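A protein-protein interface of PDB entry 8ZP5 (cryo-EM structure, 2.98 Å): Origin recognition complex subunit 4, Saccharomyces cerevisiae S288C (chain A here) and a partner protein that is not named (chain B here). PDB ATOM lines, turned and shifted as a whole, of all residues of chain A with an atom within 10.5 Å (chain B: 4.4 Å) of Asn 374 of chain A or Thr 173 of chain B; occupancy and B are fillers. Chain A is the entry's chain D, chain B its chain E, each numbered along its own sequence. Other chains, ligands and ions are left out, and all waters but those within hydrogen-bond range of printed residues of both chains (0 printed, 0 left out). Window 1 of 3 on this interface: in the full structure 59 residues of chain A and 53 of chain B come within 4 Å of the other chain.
Among the printed residues, pairs that only touch across the chains: Ser 373 of chain A with Pro 190 of chain B (3.1 Å), Leu 477 of chain A with Phe 175 of chain B (3.4 Å), Arg 379 of chain A with Thr 173 of chain B (3.5 Å), Gln 465 of chain A with Glu 172 of chain B (3.5 Å), Asn 374 of chain A with Thr 173 of chain B (3.6 Å), Leu 466 of chain A with Tyr 38 of chain B (3.7 Å), Asn 374 of chain A with Phe 189 of chain B (3.8 Å), Asn 374 of chain A with Tyr 38 of chain B (3.8 Å) and Gln 371 of chain A with Met 188 of chain B (3.9 Å).
Hydrophobic or aromatic side chains of chain B within 4 Å of the printed part of chain A: Tyr 38, Phe 175, Met 188 and Pro 190.
Printed residues of chain A that touch a printed residue of chain B: Asn 370, Gln 371, Ser 373, Asn 374, Arg 379, Gln 465, Leu 466, Asp 467 and Leu 477.
Hydrophobic or aromatic side chains of chain A within 4 Å of the printed part of chain B: Leu 466 and Leu 477.
Along chain A the printed residues that touch a printed residue of chain B span positions 370 to 477.
The side-chain sulfur (SD) of Met 188 of chain B lies close to the side-chain amide oxygen (OD1) of Asn 374 of chain A, 3.6 Å away.
The side-chain amide oxygen of Gln 36 of chain B sits close to the side-chain amide oxygen of Asn 374 of chain A (3.0 Å).
OD2 of Asp 467 of chain A lies close to OE2 of Glu 172 of chain B (2.8 Å).
The backbone carbonyl oxygen of Met 188 of chain B is in hydrogen-bond range of the side-chain amide nitrogen of Asn 370 of chain A, at 3.1 Å.
NE of Arg 379 of chain A lies close to OH of Tyr 38 of chain B (3.3 Å).
The side-chain amide nitrogen (NE2) of Gln 36 of chain B lies within hydrogen-bond range of the backbone carbonyl oxygen (O) of Leu 171 of chain B (3.1 Å).
NE2 of Gln 36 of chain B lies close to N of Thr 173 of chain B.
O of Asn 375 of chain A lies close to NE of Arg 379 of chain A.
The side-chain amide oxygen of Gln 36 of chain B lies close to the side-chain sulfur of Met 188 of chain B (3.4 Å).
O of Gln 36 of chain B lies within hydrogen-bond range of N of Phe 189 of chain B, at 2.9 Å.
OH of Tyr 38 of chain B is in hydrogen-bond range of OE2 of Glu 172 of chain B (3.0 Å).
Asn 374 of chain A touches five residues of chain B.
Thr 173 of chain B touches just these residues of chain A: Asn 374 and Arg 379.
Glu 172 of chain B touches just these residues of chain A: Gln 465 and Asp 467.
No residue of chain A comes within 4 Å of Ser 174 of chain B.
No residue of chain A comes within 4 Å of Leu 176 of chain B.
No residue of chain A comes within 4 Å of Gln 177 of chain B.
Of the printed residues of chain A, Phe 175 of chain B touches Leu 477 (3.4 Å).
Of the printed residues of chain B, Asp 467 of chain A touches Glu 172 (2.8 Å).
Printed residues of chain B within 4 Å of Arg 379 of chain A: Tyr 38 (3.2 Å) and Thr 173 (3.5 Å).
Val 464 of chain A touches none of the printed residues of chain B.
The nearest residue of chain B that does not touch Asn 374 of chain A is Pro 190 of chain B (4.2 Å).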
ATOM      1  N   TYR A 367     -25.357   0.896  10.462  1.00  0.00           N
ATOM      2  CA  TYR A 367     -24.800  -0.435  10.248  1.00  0.00           C
ATOM      3  C   TYR A 367     -24.774  -0.788   8.769  1.00  0.00           C
ATOM      4  O   TYR A 367     -23.778  -1.324   8.269  1.00  0.00           O
ATOM      5  CB  TYR A 367     -25.616  -1.458  11.041  1.00  0.00           C
ATOM      6  CG  TYR A 367     -25.207  -2.901  10.855  1.00  0.00           C
ATOM      7  CD1 TYR A 367     -24.226  -3.472  11.651  1.00  0.00           C
ATOM      8  CD2 TYR A 367     -25.821  -3.700   9.903  1.00  0.00           C
ATOM      9  CE1 TYR A 367     -23.855  -4.791  11.491  1.00  0.00           C
ATOM     10  CE2 TYR A 367     -25.456  -5.020   9.735  1.00  0.00           C
ATOM     11  CZ  TYR A 367     -24.474  -5.560  10.532  1.00  0.00           C
ATOM     12  OH  TYR A 367     -24.108  -6.876  10.370  1.00  0.00           O
ATOM     13  N   ASN A 368     -25.859  -0.490   8.051  1.00  0.00           N
ATOM     14  CA  ASN A 368     -25.903  -0.781   6.623  1.00  0.00           C
ATOM     15  C   ASN A 368     -24.868   0.034   5.859  1.00  0.00           C
ATOM     16  O   ASN A 368     -24.223  -0.476   4.938  1.00  0.00           O
ATOM     17  CB  ASN A 368     -27.304  -0.517   6.080  1.00  0.00           C
ATOM     18  CG  ASN A 368     -28.338  -1.462   6.653  1.00  0.00           C
ATOM     19  OD1 ASN A 368     -28.051  -2.629   6.913  1.00  0.00           O
ATOM     20  ND2 ASN A 368     -29.550  -0.961   6.852  1.00  0.00           N
ATOM     21  N   LYS A 369     -24.701   1.308   6.223  1.00  0.00           N
ATOM     22  CA  LYS A 369     -23.681   2.133   5.586  1.00  0.00           C
ATOM     23  C   LYS A 369     -22.286   1.588   5.852  1.00  0.00           C
ATOM     24  O   LYS A 369     -21.436   1.572   4.956  1.00  0.00           O
ATOM     25  CB  LYS A 369     -23.790   3.575   6.078  1.00  0.00           C
ATOM     26  CG  LYS A 369     -22.679   4.483   5.587  1.00  0.00           C
ATOM     27  CD  LYS A 369     -22.849   5.894   6.117  1.00  0.00           C
ATOM     28  CE  LYS A 369     -21.666   6.768   5.740  1.00  0.00           C
ATOM     29  NZ  LYS A 369     -21.591   6.998   4.271  1.00  0.00           N
ATOM     30  N   ASN A 370     -22.029   1.140   7.083  1.00  0.00           N
ATOM     31  CA  ASN A 370     -20.714   0.600   7.411  1.00  0.00           C
ATOM     32  C   ASN A 370     -20.441  -0.699   6.666  1.00  0.00           C
ATOM     33  O   ASN A 370     -19.311  -0.942   6.229  1.00  0.00           O
ATOM     34  CB  ASN A 370     -20.592   0.388   8.916  1.00  0.00           C
ATOM     35  CG  ASN A 370     -19.370  -0.422   9.290  1.00  0.00           C
ATOM     36  OD1 ASN A 370     -19.431  -1.646   9.388  1.00  0.00           O
ATOM     37  ND2 ASN A 370     -18.252   0.258   9.504  1.00  0.00           N
ATOM     38  N   GLN A 371     -21.460  -1.551   6.514  1.00  0.00           N
ATOM     39  CA  GLN A 371     -21.255  -2.823   5.828  1.00  0.00           C
ATOM     40  C   GLN A 371     -20.845  -2.622   4.375  1.00  0.00           C
ATOM     41  O   GLN A 371     -20.134  -3.460   3.809  1.00  0.00           O
ATOM     42  CB  GLN A 371     -22.522  -3.675   5.907  1.00  0.00           C
ATOM     43  CG  GLN A 371     -22.830  -4.213   7.293  1.00  0.00           C
ATOM     44  CD  GLN A 371     -21.824  -5.242   7.760  1.00  0.00           C
ATOM     45  OE1 GLN A 371     -21.021  -4.980   8.653  1.00  0.00           O
ATOM     46  NE2 GLN A 371     -21.863  -6.423   7.158  1.00  0.00           N
ATOM     47  N   LEU A 372     -21.277  -1.523   3.757  1.00  0.00           N
ATOM     48  CA  LEU A 372     -20.967  -1.215   2.367  1.00  0.00           C
ATOM     49  C   LEU A 372     -19.833  -0.205   2.239  1.00  0.00           C
ATOM     50  O   LEU A 372     -19.846   0.629   1.327  1.00  0.00           O
ATOM     51  CB  LEU A 372     -22.214  -0.696   1.652  1.00  0.00           C
ATOM     52  CG  LEU A 372     -23.488  -1.527   1.777  1.00  0.00           C
ATOM     53  CD1 LEU A 372     -24.693  -0.707   1.360  1.00  0.00           C
ATOM     54  CD2 LEU A 372     -23.384  -2.790   0.945  1.00  0.00           C
ATOM     55  N   SER A 373     -18.853  -0.255   3.139  1.00  0.00           N
ATOM     56  CA  SER A 373     -17.803   0.751   3.190  1.00  0.00           C
ATOM     57  C   SER A 373     -16.452   0.246   2.703  1.00  0.00           C
ATOM     58  O   SER A 373     -15.482   1.009   2.720  1.00  0.00           O
ATOM     59  CB  SER A 373     -17.664   1.291   4.617  1.00  0.00           C
ATOM     60  OG  SER A 373     -16.679   2.302   4.676  1.00  0.00           O
ATOM     61  N   ASN A 374     -16.356  -1.013   2.272  1.00  0.00           N
ATOM     62  CA  ASN A 374     -15.110  -1.548   1.739  1.00  0.00           C
ATOM     63  C   ASN A 374     -15.275  -2.142   0.346  1.00  0.00           C
ATOM     64  O   ASN A 374     -14.334  -2.760  -0.163  1.00  0.00           O
ATOM     65  CB  ASN A 374     -14.522  -2.604   2.680  1.00  0.00           C
ATOM     66  CG  ASN A 374     -13.827  -1.994   3.878  1.00  0.00           C
ATOM     67  OD1 ASN A 374     -14.237  -2.199   5.019  1.00  0.00           O
ATOM     68  ND2 ASN A 374     -12.766  -1.238   3.625  1.00  0.00           N
ATOM     69  N   ASN A 375     -16.434  -1.975  -0.281  1.00  0.00           N
ATOM     70  CA  ASN A 375     -16.648  -2.479  -1.630  1.00  0.00           C
ATOM     71  C   ASN A 375     -16.022  -1.511  -2.632  1.00  0.00           C
ATOM     72  O   ASN A 375     -15.231  -0.634  -2.274  1.00  0.00           O
ATOM     73  CB  ASN A 375     -18.136  -2.702  -1.883  1.00  0.00           C
ATOM     74  CG  ASN A 375     -18.975  -1.507  -1.500  1.00  0.00           C
ATOM     75  OD1 ASN A 375     -18.485  -0.565  -0.880  1.00  0.00           O
ATOM     76  ND2 ASN A 375     -20.248  -1.535  -1.870  1.00  0.00           N
ATOM     77  N   LEU A 376     -16.366  -1.669  -3.913  1.00  0.00           N
ATOM     78  CA  LEU A 376     -15.733  -0.866  -4.956  1.00  0.00           C
ATOM     79  C   LEU A 376     -15.998   0.621  -4.763  1.00  0.00           C
ATOM     80  O   LEU A 376     -15.087   1.442  -4.915  1.00  0.00           O
ATOM     81  CB  LEU A 376     -16.217  -1.321  -6.332  1.00  0.00           C
ATOM     82  CG  LEU A 376     -15.510  -2.531  -6.939  1.00  0.00           C
ATOM     83  CD1 LEU A 376     -16.090  -2.848  -8.305  1.00  0.00           C
ATOM     84  CD2 LEU A 376     -14.012  -2.289  -7.029  1.00  0.00           C
ATOM     85  N   THR A 377     -17.236   0.991  -4.430  1.00  0.00           N
ATOM     86  CA  THR A 377     -17.558   2.403  -4.247  1.00  0.00           C
ATOM     87  C   THR A 377     -16.845   2.979  -3.029  1.00  0.00           C
ATOM     88  O   THR A 377     -16.256   4.066  -3.096  1.00  0.00           O
ATOM     89  CB  THR A 377     -19.070   2.584  -4.117  1.00  0.00           C
ATOM     90  OG1 THR A 377     -19.732   1.808  -5.122  1.00  0.00           O
ATOM     91  CG2 THR A 377     -19.444   4.045  -4.285  1.00  0.00           C
ATOM     92  N   GLY A 378     -16.883   2.261  -1.905  1.00  0.00           N
ATOM     93  CA  GLY A 378     -16.231   2.751  -0.703  1.00  0.00           C
ATOM     94  C   GLY A 378     -14.726   2.852  -0.852  1.00  0.00           C
ATOM     95  O   GLY A 378     -14.108   3.806  -0.374  1.00  0.00           O
ATOM     96  N   ARG A 379     -14.111   1.865  -1.508  1.00  0.00           N
ATOM     97  CA  ARG A 379     -12.674   1.924  -1.750  1.00  0.00           C
ATOM     98  C   ARG A 379     -12.322   3.040  -2.725  1.00  0.00           C
ATOM     99  O   ARG A 379     -11.308   3.724  -2.553  1.00  0.00           O
ATOM    100  CB  ARG A 379     -12.175   0.582  -2.278  1.00  0.00           C
ATOM    101  CG  ARG A 379     -11.723  -0.379  -1.204  1.00  0.00           C
ATOM    102  CD  ARG A 379     -11.294  -1.692  -1.821  1.00  0.00           C
ATOM    103  NE  ARG A 379     -12.439  -2.499  -2.225  1.00  0.00           N
ATOM    104  CZ  ARG A 379     -12.422  -3.373  -3.220  1.00  0.00           C
ATOM    105  NH1 ARG A 379     -11.337  -3.570  -3.949  1.00  0.00           N
ATOM    106  NH2 ARG A 379     -13.523  -4.066  -3.494  1.00  0.00           N
ATOM    107  N   LEU A 380     -13.145   3.231  -3.759  1.00  0.00           N
ATOM    108  CA  LEU A 380     -12.889   4.289  -4.729  1.00  0.00           C
ATOM    109  C   LEU A 380     -12.987   5.664  -4.084  1.00  0.00           C
ATOM    110  O   LEU A 380     -12.231   6.578  -4.432  1.00  0.00           O
ATOM    111  CB  LEU A 380     -13.867   4.175  -5.897  1.00  0.00           C
ATOM    112  CG  LEU A 380     -13.801   5.282  -6.947  1.00  0.00           C
ATOM    113  CD1 LEU A 380     -12.398   5.402  -7.510  1.00  0.00           C
ATOM    114  CD2 LEU A 380     -14.796   5.020  -8.053  1.00  0.00           C
ATOM    115  N   GLN A 381     -13.909   5.831  -3.139  1.00  0.00           N
ATOM    116  CA  GLN A 381     -14.043   7.121  -2.471  1.00  0.00           C
ATOM    117  C   GLN A 381     -12.923   7.399  -1.478  1.00  0.00           C
ATOM    118  O   GLN A 381     -12.979   8.424  -0.789  1.00  0.00           O
ATOM    119  CB  GLN A 381     -15.395   7.208  -1.766  1.00  0.00           C
ATOM    120  CG  GLN A 381     -16.570   7.341  -2.715  1.00  0.00           C
ATOM    121  CD  GLN A 381     -17.900   7.341  -1.997  1.00  0.00           C
ATOM    122  OE1 GLN A 381     -17.955   7.371  -0.768  1.00  0.00           O
ATOM    123  NE2 GLN A 381     -18.983   7.310  -2.761  1.00  0.00           N
ATOM    124  N   SER A 382     -11.918   6.533  -1.383  1.00  0.00           N
ATOM    125  CA  SER A 382     -10.788   6.711  -0.480  1.00  0.00           C
ATOM    126  C   SER A 382      -9.468   6.673  -1.240  1.00  0.00           C
ATOM    127  O   SER A 382      -8.478   6.107  -0.772  1.00  0.00           O
ATOM    128  CB  SER A 382     -10.802   5.655   0.622  1.00  0.00           C
ATOM    129  OG  SER A 382     -11.685   6.022   1.668  1.00  0.00           O
ATOM    130  N   VAL A 464      -3.231  -2.150  -7.101  1.00  0.00           N
ATOM    131  CA  VAL A 464      -3.319  -3.599  -7.247  1.00  0.00           C
ATOM    132  C   VAL A 464      -3.687  -4.249  -5.917  1.00  0.00           C
ATOM    133  O   VAL A 464      -4.450  -5.222  -5.876  1.00  0.00           O
ATOM    134  CB  VAL A 464      -2.000  -4.157  -7.815  1.00  0.00           C
ATOM    135  CG1 VAL A 464      -1.958  -5.671  -7.695  1.00  0.00           C
ATOM    136  CG2 VAL A 464      -1.834  -3.738  -9.265  1.00  0.00           C
ATOM    137  N   GLN A 465      -3.164  -3.716  -4.809  1.00  0.00           N
ATOM    138  CA  GLN A 465      -3.459  -4.282  -3.496  1.00  0.00           C
ATOM    139  C   GLN A 465      -4.943  -4.177  -3.164  1.00  0.00           C
ATOM    140  O   GLN A 465      -5.526  -5.109  -2.599  1.00  0.00           O
ATOM    141  CB  GLN A 465      -2.624  -3.588  -2.422  1.00  0.00           C
ATOM    142  CG  GLN A 465      -1.220  -4.143  -2.275  1.00  0.00           C
ATOM    143  CD  GLN A 465      -0.487  -3.560  -1.086  1.00  0.00           C
ATOM    144  OE1 GLN A 465      -1.065  -2.830  -0.282  1.00  0.00           O
ATOM    145  NE2 GLN A 465       0.797  -3.880  -0.968  1.00  0.00           N
ATOM    146  N   LEU A 466      -5.570  -3.053  -3.504  1.00  0.00           N
ATOM    147  CA  LEU A 466      -7.001  -2.872  -3.295  1.00  0.00           C
ATOM    148  C   LEU A 466      -7.844  -3.641  -4.304  1.00  0.00           C
ATOM    149  O   LEU A 466      -9.066  -3.464  -4.330  1.00  0.00           O
ATOM    150  CB  LEU A 466      -7.357  -1.384  -3.355  1.00  0.00           C
ATOM    151  CG  LEU A 466      -6.600  -0.458  -2.404  1.00  0.00           C
ATOM    152  CD1 LEU A 466      -7.139   0.958  -2.496  1.00  0.00           C
ATOM    153  CD2 LEU A 466      -6.683  -0.970  -0.980  1.00  0.00           C
ATOM    154  N   ASP A 467      -7.216  -4.487  -5.121  1.00  0.00           N
ATOM    155  CA  ASP A 467      -7.888  -5.243  -6.177  1.00  0.00           C
ATOM    156  C   ASP A 467      -8.756  -4.347  -7.053  1.00  0.00           C
ATOM    157  O   ASP A 467      -9.925  -4.632  -7.321  1.00  0.00           O
ATOM    158  CB  ASP A 467      -8.693  -6.408  -5.602  1.00  0.00           C
ATOM    159  CG  ASP A 467      -7.808  -7.499  -5.032  1.00  0.00           C
ATOM    160  OD1 ASP A 467      -6.672  -7.659  -5.527  1.00  0.00           O
ATOM    161  OD2 ASP A 467      -8.250  -8.214  -4.112  1.00  0.00           O
ATOM    162  N   PHE A 468      -8.169  -3.238  -7.495  1.00  0.00           N
ATOM    163  CA  PHE A 468      -8.704  -2.513  -8.637  1.00  0.00           C
ATOM    164  C   PHE A 468      -8.187  -3.087  -9.946  1.00  0.00           C
ATOM    165  O   PHE A 468      -8.860  -2.975 -10.976  1.00  0.00           O
ATOM    166  CB  PHE A 468      -8.352  -1.028  -8.539  1.00  0.00           C
ATOM    167  CG  PHE A 468      -9.230  -0.259  -7.596  1.00  0.00           C
ATOM    168  CD1 PHE A 468     -10.584  -0.129  -7.842  1.00  0.00           C
ATOM    169  CD2 PHE A 468      -8.700   0.336  -6.467  1.00  0.00           C
ATOM    170  CE1 PHE A 468     -11.393   0.577  -6.978  1.00  0.00           C
ATOM    171  CE2 PHE A 468      -9.506   1.042  -5.599  1.00  0.00           C
ATOM    172  CZ  PHE A 468     -10.853   1.163  -5.856  1.00  0.00           C
ATOM    173  N   LEU A 477      -8.338 -17.708  -5.436  1.00  0.00           N
ATOM    174  CA  LEU A 477      -8.064 -18.696  -4.404  1.00  0.00           C
ATOM    175  C   LEU A 477      -8.599 -20.048  -4.847  1.00  0.00           C
ATOM    176  O   LEU A 477      -9.753 -20.154  -5.274  1.00  0.00           O
ATOM    177  CB  LEU A 477      -8.684 -18.293  -3.065  1.00  0.00           C
ATOM    178  CG  LEU A 477      -7.894 -17.255  -2.269  1.00  0.00           C
ATOM    179  CD1 LEU A 477      -8.493 -17.088  -0.894  1.00  0.00           C
ATOM    180  CD2 LEU A 477      -6.433 -17.659  -2.171  1.00  0.00           C
ATOM    181  N   GLN A 507     -11.255  -4.472 -12.488  1.00  0.00           N
ATOM    182  CA  GLN A 507     -12.525  -4.896 -11.924  1.00  0.00           C
ATOM    183  C   GLN A 507     -13.598  -3.824 -12.006  1.00  0.00           C
ATOM    184  O   GLN A 507     -14.783  -4.149 -11.883  1.00  0.00           O
ATOM    185  CB  GLN A 507     -12.346  -5.301 -10.454  1.00  0.00           C
ATOM    186  CG  GLN A 507     -11.507  -6.546 -10.251  1.00  0.00           C
ATOM    187  CD  GLN A 507     -11.572  -7.058  -8.830  1.00  0.00           C
ATOM    188  OE1 GLN A 507     -12.248  -6.478  -7.981  1.00  0.00           O
ATOM    189  NE2 GLN A 507     -10.866  -8.149  -8.559  1.00  0.00           N
ATOM    190  N   GLN B  36     -13.006  -6.578   9.328  1.00  0.00           N
ATOM    191  CA  GLN B  36     -12.547  -6.440   7.954  1.00  0.00           C
ATOM    192  C   GLN B  36     -11.974  -5.049   7.736  1.00  0.00           C
ATOM    193  O   GLN B  36     -12.409  -4.080   8.359  1.00  0.00           O
ATOM    194  CB  GLN B  36     -13.677  -6.699   6.955  1.00  0.00           C
ATOM    195  CG  GLN B  36     -13.200  -7.250   5.624  1.00  0.00           C
ATOM    196  CD  GLN B  36     -12.926  -6.164   4.607  1.00  0.00           C
ATOM    197  OE1 GLN B  36     -13.577  -5.122   4.606  1.00  0.00           O
ATOM    198  NE2 GLN B  36     -11.956  -6.402   3.735  1.00  0.00           N
ATOM    199  N   TYR B  38      -8.445  -2.872   5.367  1.00  0.00           N
ATOM    200  CA  TYR B  38      -7.178  -2.935   4.659  1.00  0.00           C
ATOM    201  C   TYR B  38      -6.038  -2.494   5.572  1.00  0.00           C
ATOM    202  O   TYR B  38      -6.225  -2.222   6.759  1.00  0.00           O
ATOM    203  CB  TYR B  38      -7.247  -2.095   3.384  1.00  0.00           C
ATOM    204  CG  TYR B  38      -8.105  -2.737   2.321  1.00  0.00           C
ATOM    205  CD1 TYR B  38      -7.561  -3.633   1.416  1.00  0.00           C
ATOM    206  CD2 TYR B  38      -9.461  -2.467   2.240  1.00  0.00           C
ATOM    207  CE1 TYR B  38      -8.338  -4.230   0.452  1.00  0.00           C
ATOM    208  CE2 TYR B  38     -10.248  -3.063   1.278  1.00  0.00           C
ATOM    209  CZ  TYR B  38      -9.681  -3.944   0.388  1.00  0.00           C
ATOM    210  OH  TYR B  38     -10.458  -4.540  -0.576  1.00  0.00           O
ATOM    211  N   LEU B 171      -8.210  -9.155   5.675  1.00  0.00           N
ATOM    212  CA  LEU B 171      -7.676  -8.008   4.952  1.00  0.00           C
ATOM    213  C   LEU B 171      -8.496  -7.645   3.720  1.00  0.00           C
ATOM    214  O   LEU B 171      -8.873  -6.483   3.550  1.00  0.00           O
ATOM    215  CB  LEU B 171      -6.223  -8.280   4.546  1.00  0.00           C
ATOM    216  CG  LEU B 171      -5.360  -7.051   4.271  1.00  0.00           C
ATOM    217  CD1 LEU B 171      -4.845  -6.468   5.572  1.00  0.00           C
ATOM    218  CD2 LEU B 171      -4.207  -7.405   3.351  1.00  0.00           C
ATOM    219  N   GLU B 172      -8.784  -8.612   2.856  1.00  0.00           N
ATOM    220  CA  GLU B 172      -9.412  -8.351   1.570  1.00  0.00           C
ATOM    221  C   GLU B 172     -10.904  -8.649   1.631  1.00  0.00           C
ATOM    222  O   GLU B 172     -11.325  -9.647   2.221  1.00  0.00           O
ATOM    223  CB  GLU B 172      -8.762  -9.186   0.464  1.00  0.00           C
ATOM    224  CG  GLU B 172      -9.345  -8.927  -0.912  1.00  0.00           C
ATOM    225  CD  GLU B 172      -9.085  -7.514  -1.397  1.00  0.00           C
ATOM    226  OE1 GLU B 172      -8.091  -6.905  -0.953  1.00  0.00           O
ATOM    227  OE2 GLU B 172      -9.884  -7.008  -2.214  1.00  0.00           O
ATOM    228  N   THR B 173     -11.699  -7.772   1.013  1.00  0.00           N
ATOM    229  CA  THR B 173     -13.142  -7.975   0.956  1.00  0.00           C
ATOM    230  C   THR B 173     -13.536  -9.055  -0.043  1.00  0.00           C
ATOM    231  O   THR B 173     -14.606  -9.657   0.096  1.00  0.00           O
ATOM    232  CB  THR B 173     -13.851  -6.664   0.611  1.00  0.00           C
ATOM    233  OG1 THR B 173     -15.265  -6.883   0.559  1.00  0.00           O
ATOM    234  CG2 THR B 173     -13.379  -6.137  -0.729  1.00  0.00           C
ATOM    235  N   SER B 174     -12.699  -9.312  -1.051  1.00  0.00           N
ATOM    236  CA  SER B 174     -13.009 -10.363  -2.015  1.00  0.00           C
ATOM    237  C   SER B 174     -13.008 -11.732  -1.350  1.00  0.00           C
ATOM    238  O   SER B 174     -13.785 -12.617  -1.729  1.00  0.00           O
ATOM    239  CB  SER B 174     -12.013 -10.328  -3.172  1.00  0.00           C
ATOM    240  OG  SER B 174     -10.831 -11.040  -2.846  1.00  0.00           O
ATOM    241  N   PHE B 175     -12.135 -11.928  -0.362  1.00  0.00           N
ATOM    242  CA  PHE B 175     -12.137 -13.177   0.390  1.00  0.00           C
ATOM    243  C   PHE B 175     -13.333 -13.259   1.326  1.00  0.00           C
ATOM    244  O   PHE B 175     -13.950 -14.323   1.462  1.00  0.00           O
ATOM    245  CB  PHE B 175     -10.834 -13.314   1.173  1.00  0.00           C
ATOM    246  CG  PHE B 175     -10.724 -14.590   1.950  1.00  0.00           C
ATOM    247  CD1 PHE B 175     -10.772 -15.812   1.309  1.00  0.00           C
ATOM    248  CD2 PHE B 175     -10.568 -14.566   3.321  1.00  0.00           C
ATOM    249  CE1 PHE B 175     -10.667 -16.986   2.023  1.00  0.00           C
ATOM    250  CE2 PHE B 175     -10.463 -15.735   4.040  1.00  0.00           C
ATOM    251  CZ  PHE B 175     -10.513 -16.947   3.391  1.00  0.00           C
ATOM    252  N   LEU B 176     -13.672 -12.150   1.987  1.00  0.00           N
ATOM    253  CA  LEU B 176     -14.790 -12.159   2.924  1.00  0.00           C
ATOM    254  C   LEU B 176     -16.108 -12.421   2.209  1.00  0.00           C
ATOM    255  O   LEU B 176     -16.964 -13.152   2.718  1.00  0.00           O
ATOM    256  CB  LEU B 176     -14.849 -10.836   3.686  1.00  0.00           C
ATOM    257  CG  LEU B 176     -16.173 -10.514   4.384  1.00  0.00           C
ATOM    258  CD1 LEU B 176     -16.483 -11.532   5.470  1.00  0.00           C
ATOM    259  CD2 LEU B 176     -16.160  -9.111   4.953  1.00  0.00           C
ATOM    260  N   GLN B 177     -16.288 -11.840   1.022  1.00  0.00           N
ATOM    261  CA  GLN B 177     -17.547 -11.984   0.305  1.00  0.00           C
ATOM    262  C   GLN B 177     -17.811 -13.412  -0.151  1.00  0.00           C
ATOM    263  O   GLN B 177     -18.943 -13.715  -0.538  1.00  0.00           O
ATOM    264  CB  GLN B 177     -17.575 -11.041  -0.896  1.00  0.00           C
ATOM    265  CG  GLN B 177     -17.866  -9.597  -0.530  1.00  0.00           C
ATOM    266  CD  GLN B 177     -17.910  -8.687  -1.738  1.00  0.00           C
ATOM    267  OE1 GLN B 177     -17.245  -8.939  -2.744  1.00  0.00           O
ATOM    268  NE2 GLN B 177     -18.700  -7.624  -1.650  1.00  0.00           N
ATOM    269  N   MET B 188     -16.643  -3.379   9.909  1.00  0.00           N
ATOM    270  CA  MET B 188     -15.865  -2.857   8.797  1.00  0.00           C
ATOM    271  C   MET B 188     -15.005  -1.692   9.263  1.00  0.00           C
ATOM    272  O   MET B 188     -15.424  -0.892  10.103  1.00  0.00           O
ATOM    273  CB  MET B 188     -16.783  -2.400   7.665  1.00  0.00           C
ATOM    274  CG  MET B 188     -17.578  -3.514   7.016  1.00  0.00           C
ATOM    275  SD  MET B 188     -16.571  -4.745   6.183  1.00  0.00           S
ATOM    276  CE  MET B 188     -17.823  -5.958   5.784  1.00  0.00           C
ATOM    277  N   PHE B 189     -13.798  -1.600   8.707  1.00  0.00           N
ATOM    278  CA  PHE B 189     -12.842  -0.547   9.037  1.00  0.00           C
ATOM    279  C   PHE B 189     -12.508   0.203   7.755  1.00  0.00           C
ATOM    280  O   PHE B 189     -11.581  -0.182   7.025  1.00  0.00           O
ATOM    281  CB  PHE B 189     -11.585  -1.131   9.680  1.00  0.00           C
ATOM    282  CG  PHE B 189     -11.773  -1.558  11.108  1.00  0.00           C
ATOM    283  CD1 PHE B 189     -12.367  -2.767  11.410  1.00  0.00           C
ATOM    284  CD2 PHE B 189     -11.347  -0.751  12.146  1.00  0.00           C
ATOM    285  CE1 PHE B 189     -12.540  -3.161  12.720  1.00  0.00           C
ATOM    286  CE2 PHE B 189     -11.516  -1.143  13.457  1.00  0.00           C
ATOM    287  CZ  PHE B 189     -12.114  -2.347  13.742  1.00  0.00           C
ATOM    288  N   PRO B 190     -13.244   1.262   7.432  1.00  0.00           N
ATOM    289  CA  PRO B 190     -12.922   2.043   6.236  1.00  0.00           C
ATOM    290  C   PRO B 190     -11.565   2.715   6.357  1.00  0.00           C
ATOM    291  O   PRO B 190     -11.101   3.044   7.451  1.00  0.00           O
ATOM    292  CB  PRO B 190     -14.048   3.080   6.173  1.00  0.00           C
ATOM    293  CG  PRO B 190     -14.595   3.138   7.556  1.00  0.00           C
ATOM    294  CD  PRO B 190     -14.454   1.757   8.105  1.00  0.00           C
